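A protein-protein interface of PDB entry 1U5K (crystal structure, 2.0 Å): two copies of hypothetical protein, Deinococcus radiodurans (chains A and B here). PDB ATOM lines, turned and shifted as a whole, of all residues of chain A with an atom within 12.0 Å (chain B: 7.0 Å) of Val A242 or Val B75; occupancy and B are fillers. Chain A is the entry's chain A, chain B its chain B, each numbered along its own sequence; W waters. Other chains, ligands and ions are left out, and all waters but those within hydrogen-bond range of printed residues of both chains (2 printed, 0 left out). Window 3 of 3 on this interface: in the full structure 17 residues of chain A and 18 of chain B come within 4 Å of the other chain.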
ATOM      1  N   PRO A 237      40.643  19.162 -11.685  1.00  0.00           N
ATOM      2  CA  PRO A 237      39.446  18.562 -11.074  1.00  0.00           C
ATOM      3  C   PRO A 237      38.608  19.605 -10.338  1.00  0.00           C
ATOM      4  O   PRO A 237      39.165  20.379  -9.562  1.00  0.00           O
ATOM      5  CB  PRO A 237      40.010  17.566 -10.056  1.00  0.00           C
ATOM      6  CG  PRO A 237      41.345  17.188 -10.597  1.00  0.00           C
ATOM      7  CD  PRO A 237      41.852  18.388 -11.360  1.00  0.00           C
ATOM      8  N   SER A 238      37.313  19.631 -10.631  1.00  0.00           N
ATOM      9  CA  SER A 238      36.393  20.675 -10.187  1.00  0.00           C
ATOM     10  C   SER A 238      34.961  20.187  -9.936  1.00  0.00           C
ATOM     11  O   SER A 238      34.030  20.997  -9.887  1.00  0.00           O
ATOM     12  CB  SER A 238      36.363  21.770 -11.255  1.00  0.00           C
ATOM     13  OG  SER A 238      37.692  22.162 -11.571  1.00  0.00           O
ATOM     14  N   GLY A 239      34.799  18.877  -9.770  1.00  0.00           N
ATOM     15  CA  GLY A 239      33.502  18.255  -9.582  1.00  0.00           C
ATOM     16  C   GLY A 239      33.245  17.079 -10.508  1.00  0.00           C
ATOM     17  O   GLY A 239      33.835  16.983 -11.586  1.00  0.00           O
ATOM     18  N   VAL A 240      32.341  16.199 -10.082  1.00  0.00           N
ATOM     19  CA  VAL A 240      31.869  15.090 -10.908  1.00  0.00           C
ATOM     20  C   VAL A 240      30.459  15.380 -11.432  1.00  0.00           C
ATOM     21  O   VAL A 240      29.555  15.600 -10.623  1.00  0.00           O
ATOM     22  CB  VAL A 240      31.899  13.782 -10.109  1.00  0.00           C
ATOM     23  N   PRO A 241      30.266  15.402 -12.752  1.00  0.00           N
ATOM     24  CA  PRO A 241      28.943  15.631 -13.354  1.00  0.00           C
ATOM     25  C   PRO A 241      27.804  14.802 -12.748  1.00  0.00           C
ATOM     26  O   PRO A 241      28.044  13.678 -12.299  1.00  0.00           O
ATOM     27  CB  PRO A 241      29.148  15.255 -14.827  1.00  0.00           C
ATOM     28  CG  PRO A 241      30.604  15.478 -15.083  1.00  0.00           C
ATOM     29  CD  PRO A 241      31.308  15.223 -13.780  1.00  0.00           C
ATOM     30  N   VAL A 242      26.588  15.344 -12.755  1.00  0.00           N
ATOM     31  CA  VAL A 242      25.446  14.751 -12.058  1.00  0.00           C
ATOM     32  C   VAL A 242      24.958  13.435 -12.682  1.00  0.00           C
ATOM     33  O   VAL A 242      25.379  12.363 -12.239  1.00  0.00           O
ATOM     34  CB  VAL A 242      24.280  15.759 -11.897  1.00  0.00           C
ATOM     35  CG1 VAL A 242      23.106  15.146 -11.138  1.00  0.00           C
ATOM     36  CG2 VAL A 242      24.738  16.993 -11.150  1.00  0.00           C
ATOM     37  N   LEU A 243      24.078  13.495 -13.680  1.00  0.00           N
ATOM     38  CA  LEU A 243      23.482  12.288 -14.261  1.00  0.00           C
ATOM     39  C   LEU A 243      23.038  12.430 -15.721  1.00  0.00           C
ATOM     40  O   LEU A 243      22.719  13.526 -16.190  1.00  0.00           O
ATOM     41  CB  LEU A 243      22.295  11.807 -13.415  1.00  0.00           C
ATOM     42  CG  LEU A 243      22.524  10.942 -12.168  1.00  0.00           C
ATOM     43  CD1 LEU A 243      21.184  10.481 -11.601  1.00  0.00           C
ATOM     44  CD2 LEU A 243      23.429   9.736 -12.425  1.00  0.00           C
ATOM     45  N   SER A 244      23.029  11.302 -16.430  1.00  0.00           N
ATOM     46  CA  SER A 244      22.499  11.207 -17.790  1.00  0.00           C
ATOM     47  C   SER A 244      21.214  10.381 -17.782  1.00  0.00           C
ATOM     48  O   SER A 244      20.276  10.657 -18.537  1.00  0.00           O
ATOM     49  CB  SER A 244      23.529  10.568 -18.729  1.00  0.00           C
ATOM     50  OG  SER A 244      22.916   9.986 -19.868  1.00  0.00           O
ATOM     51  N   LEU B  46      32.360  22.234  -1.166  1.00  0.00           N
ATOM     52  CA  LEU B  46      31.300  22.094  -2.169  1.00  0.00           C
ATOM     53  C   LEU B  46      31.558  20.996  -3.212  1.00  0.00           C
ATOM     54  O   LEU B  46      32.703  20.622  -3.478  1.00  0.00           O
ATOM     55  CB  LEU B  46      31.037  23.441  -2.844  1.00  0.00           C
ATOM     56  N   SER B  47      30.490  20.468  -3.803  1.00  0.00           N
ATOM     57  CA  SER B  47      30.590  19.432  -4.829  1.00  0.00           C
ATOM     58  C   SER B  47      31.180  19.888  -6.176  1.00  0.00           C
ATOM     59  O   SER B  47      31.639  19.069  -6.972  1.00  0.00           O
ATOM     60  CB  SER B  47      29.204  18.826  -5.060  1.00  0.00           C
ATOM     61  OG  SER B  47      29.286  17.434  -5.284  1.00  0.00           O
ATOM     62  N   SER B  48      31.152  21.194  -6.427  1.00  0.00           N
ATOM     63  CA  SER B  48      31.698  21.837  -7.616  1.00  0.00           C
ATOM     64  C   SER B  48      32.452  23.085  -7.158  1.00  0.00           C
ATOM     65  O   SER B  48      32.007  23.825  -6.284  1.00  0.00           O
ATOM     66  CB  SER B  48      30.576  22.181  -8.608  1.00  0.00           C
ATOM     67  OG  SER B  48      30.894  23.225  -9.517  1.00  0.00           O
ATOM     68  N   LEU B  50      32.784  25.527  -9.036  1.00  0.00           N
ATOM     69  CA  LEU B  50      32.190  26.566  -9.879  1.00  0.00           C
ATOM     70  C   LEU B  50      33.134  27.114 -10.953  1.00  0.00           C
ATOM     71  O   LEU B  50      33.284  28.318 -11.117  1.00  0.00           O
ATOM     72  CB  LEU B  50      31.650  27.700  -9.003  1.00  0.00           C
ATOM     73  CG  LEU B  50      30.668  27.269  -7.910  1.00  0.00           C
ATOM     74  CD1 LEU B  50      30.488  28.342  -6.892  1.00  0.00           C
ATOM     75  CD2 LEU B  50      29.330  26.915  -8.512  1.00  0.00           C
ATOM     76  N   HIS B  55      28.375  24.542 -16.478  1.00  0.00           N
ATOM     77  CA  HIS B  55      26.949  24.578 -16.217  1.00  0.00           C
ATOM     78  C   HIS B  55      26.754  23.935 -14.855  1.00  0.00           C
ATOM     79  O   HIS B  55      27.078  22.764 -14.666  1.00  0.00           O
ATOM     80  CB  HIS B  55      26.153  23.850 -17.303  1.00  0.00           C
ATOM     81  CG  HIS B  55      24.693  24.169 -17.257  1.00  0.00           C
ATOM     82  ND1 HIS B  55      23.938  24.388 -18.389  1.00  0.00           N
ATOM     83  CD2 HIS B  55      23.860  24.338 -16.204  1.00  0.00           C
ATOM     84  CE1 HIS B  55      22.702  24.688 -18.028  1.00  0.00           C
ATOM     85  NE2 HIS B  55      22.624  24.650 -16.710  1.00  0.00           N
ATOM     86  N   VAL B  56      26.297  24.721 -13.886  1.00  0.00           N
ATOM     87  CA  VAL B  56      26.211  24.255 -12.507  1.00  0.00           C
ATOM     88  C   VAL B  56      24.803  24.441 -11.972  1.00  0.00           C
ATOM     89  O   VAL B  56      24.084  25.333 -12.410  1.00  0.00           O
ATOM     90  CB  VAL B  56      27.175  24.986 -11.551  1.00  0.00           C
ATOM     91  CG1 VAL B  56      28.615  24.718 -11.929  1.00  0.00           C
ATOM     92  CG2 VAL B  56      26.900  26.492 -11.509  1.00  0.00           C
ATOM     93  N   GLY B  57      24.416  23.566 -11.049  1.00  0.00           N
ATOM     94  CA  GLY B  57      23.230  23.761 -10.233  1.00  0.00           C
ATOM     95  C   GLY B  57      23.683  24.188  -8.847  1.00  0.00           C
ATOM     96  O   GLY B  57      24.612  23.606  -8.289  1.00  0.00           O
ATOM     97  N   VAL B  58      23.085  25.258  -8.337  1.00  0.00           N
ATOM     98  CA  VAL B  58      23.400  25.786  -7.018  1.00  0.00           C
ATOM     99  C   VAL B  58      22.139  25.937  -6.182  1.00  0.00           C
ATOM    100  O   VAL B  58      21.033  26.074  -6.696  1.00  0.00           O
ATOM    101  CB  VAL B  58      24.129  27.136  -7.064  1.00  0.00           C
ATOM    102  CG1 VAL B  58      25.463  26.980  -7.750  1.00  0.00           C
ATOM    103  CG2 VAL B  58      23.328  28.203  -7.784  1.00  0.00           C
ATOM    104  N   GLN B  59      22.329  25.868  -4.872  1.00  0.00           N
ATOM    105  CA  GLN B  59      21.349  26.378  -3.923  1.00  0.00           C
ATOM    106  C   GLN B  59      21.966  27.575  -3.218  1.00  0.00           C
ATOM    107  O   GLN B  59      23.054  27.482  -2.654  1.00  0.00           O
ATOM    108  CB  GLN B  59      21.029  25.264  -2.930  1.00  0.00           C
ATOM    109  CG  GLN B  59      20.034  25.700  -1.861  1.00  0.00           C
ATOM    110  CD  GLN B  59      19.528  24.493  -1.102  1.00  0.00           C
ATOM    111  OE1 GLN B  59      18.559  23.858  -1.534  1.00  0.00           O
ATOM    112  NE2 GLN B  59      20.238  24.120  -0.043  1.00  0.00           N
ATOM    113  N   GLN B  73      25.104  24.933  -1.709  1.00  0.00           N
ATOM    114  CA  GLN B  73      25.370  23.690  -2.425  1.00  0.00           C
ATOM    115  C   GLN B  73      25.669  24.024  -3.887  1.00  0.00           C
ATOM    116  O   GLN B  73      25.162  24.988  -4.453  1.00  0.00           O
ATOM    117  CB  GLN B  73      24.179  22.728  -2.400  1.00  0.00           C
ATOM    118  CG  GLN B  73      23.776  22.165  -1.049  1.00  0.00           C
ATOM    119  CD  GLN B  73      22.539  21.285  -1.155  1.00  0.00           C
ATOM    120  OE1 GLN B  73      22.645  20.060  -1.227  1.00  0.00           O
ATOM    121  NE2 GLN B  73      21.363  21.905  -1.178  1.00  0.00           N
ATOM    122  N   ALA B  74      26.512  23.210  -4.505  1.00  0.00           N
ATOM    123  CA  ALA B  74      26.830  23.393  -5.919  1.00  0.00           C
ATOM    124  C   ALA B  74      27.177  22.032  -6.500  1.00  0.00           C
ATOM    125  O   ALA B  74      27.980  21.316  -5.897  1.00  0.00           O
ATOM    126  CB  ALA B  74      27.975  24.383  -6.087  1.00  0.00           C
ATOM    127  N   VAL B  75      26.528  21.672  -7.607  1.00  0.00           N
ATOM    128  CA  VAL B  75      26.859  20.474  -8.375  1.00  0.00           C
ATOM    129  C   VAL B  75      27.133  20.780  -9.846  1.00  0.00           C
ATOM    130  O   VAL B  75      26.548  21.685 -10.440  1.00  0.00           O
ATOM    131  CB  VAL B  75      25.787  19.364  -8.310  1.00  0.00           C
ATOM    132  CG1 VAL B  75      25.663  18.815  -6.898  1.00  0.00           C
ATOM    133  CG2 VAL B  75      24.439  19.816  -8.836  1.00  0.00           C
ATOM    134  N   LEU B  76      28.061  20.025 -10.421  1.00  0.00           N
ATOM    135  CA  LEU B  76      28.395  20.162 -11.834  1.00  0.00           C
ATOM    136  C   LEU B  76      27.305  19.495 -12.656  1.00  0.00           C
ATOM    137  O   LEU B  76      27.031  18.316 -12.445  1.00  0.00           O
ATOM    138  CB  LEU B  76      29.737  19.499 -12.135  1.00  0.00           C
ATOM    139  CG  LEU B  76      30.225  19.701 -13.578  1.00  0.00           C
ATOM    140  CD1 LEU B  76      30.268  21.165 -13.982  1.00  0.00           C
ATOM    141  CD2 LEU B  76      31.589  19.056 -13.720  1.00  0.00           C
ATOM    142  N   GLU B  77      26.679  20.235 -13.565  1.00  0.00           N
ATOM    143  CA  GLU B  77      25.706  19.649 -14.477  1.00  0.00           C
ATOM    144  C   GLU B  77      26.327  19.300 -15.831  1.00  0.00           C
ATOM    145  O   GLU B  77      25.909  18.342 -16.467  1.00  0.00           O
ATOM    146  CB  GLU B  77      24.510  20.574 -14.662  1.00  0.00           C
ATOM    147  CG  GLU B  77      23.570  20.592 -13.467  1.00  0.00           C
ATOM    148  CD  GLU B  77      22.366  21.491 -13.687  1.00  0.00           C
ATOM    149  OE1 GLU B  77      21.779  21.528 -14.799  1.00  0.00           O
ATOM    150  OE2 GLU B  77      21.993  22.161 -12.708  1.00  0.00           O
ATOM    151  N   GLY B  78      27.316  20.064 -16.281  1.00  0.00           N
ATOM    152  CA  GLY B  78      28.064  19.692 -17.469  1.00  0.00           C
ATOM    153  C   GLY B  78      29.168  20.684 -17.773  1.00  0.00           C
ATOM    154  O   GLY B  78      29.178  21.815 -17.280  1.00  0.00           O
HETATM  155  O   HOH W   1      29.358  17.908  -8.971  1.00  0.00           O
HETATM  156  O   HOH W   2      32.774  23.071 -11.433  1.00  0.00           O
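N of Val A242 sits close to O of Leu B76 (3.0 Å).
O of Ala B74 lies close to N of Ser B47 (3.4 Å).
The side-chain hydroxyl (OG) of Ser B48 is in hydrogen-bond range of the backbone NH (N) of Leu B50, at 3.0 Å.
N of Ser B48 is in hydrogen-bond range of O of Ala B74, at 3.2 Å.
The backbone carbonyl oxygen (O) of Gly B57 is in hydrogen-bond range of the backbone NH (N) of Val B75, 2.8 Å away.
Among the printed residues, pairs that only touch across the chains: Gly A239 with Ser B47, Ser A238 with Ser B48, Pro A241 with Leu B76, Val A242 with Val B75 and Gly A239 with Leu B76.
Val A242 touches two residues of chain B.
Of chain A, only Val A242 (3.7 Å) comes within 4 Å of Val B75.
Of chain A, only Ser A238 (3.4 Å) comes within 4 Å of Ser B48.
No residue of chain A comes within 4 Å of Val B56.
Of chain A, only Gly A239 (3.7 Å), Pro A241 (3.4 Å) and Val A242 (2.9 Å) come within 4 Å of Leu B76.
No residue of chain A comes within 4 Å of Glu B77.
No residue of chain A comes within 4 Å of Gly B78.
Printed residues of chain B within 4 Å of Pro A241: Leu B76.
Printed residues of chain B within 4 Å of Ser A238: Ser B48.
Leu A243 touches none of the printed residues of chain B.
The nearest residue of chain A that does not touch Val B75 is Val A240 (5.8 Å).
Of the 8 printed residues of chain A, 4 touch a printed residue of chain B.
Hydrophobic or aromatic side chains of chain A that line the printed part of chain B: Pro A241 and Val A242.
Printed residues of chain B that touch a printed residue of chain A: Ser B47, Ser B48, Val B75 and Leu B76.
Among the printed residues, no Asp or Glu carboxylate lies within 4 Å of a Lys or Arg side-chain nitrogen of the other chain.
No position is printed for both chains.
Of the 6 pairs that touch across the chains among the printed residues, none has its exchanged pair printed and touching as well.
Water W2 lies within hydrogen-bond range of OG of Ser B48, O of Ser A238 and N of Leu B50.
Water W1 lies within hydrogen-bond range of O of Val A240 (2.8 Å), N of Leu B76 (2.9 Å) and O of Ser B47 (3.2 Å).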
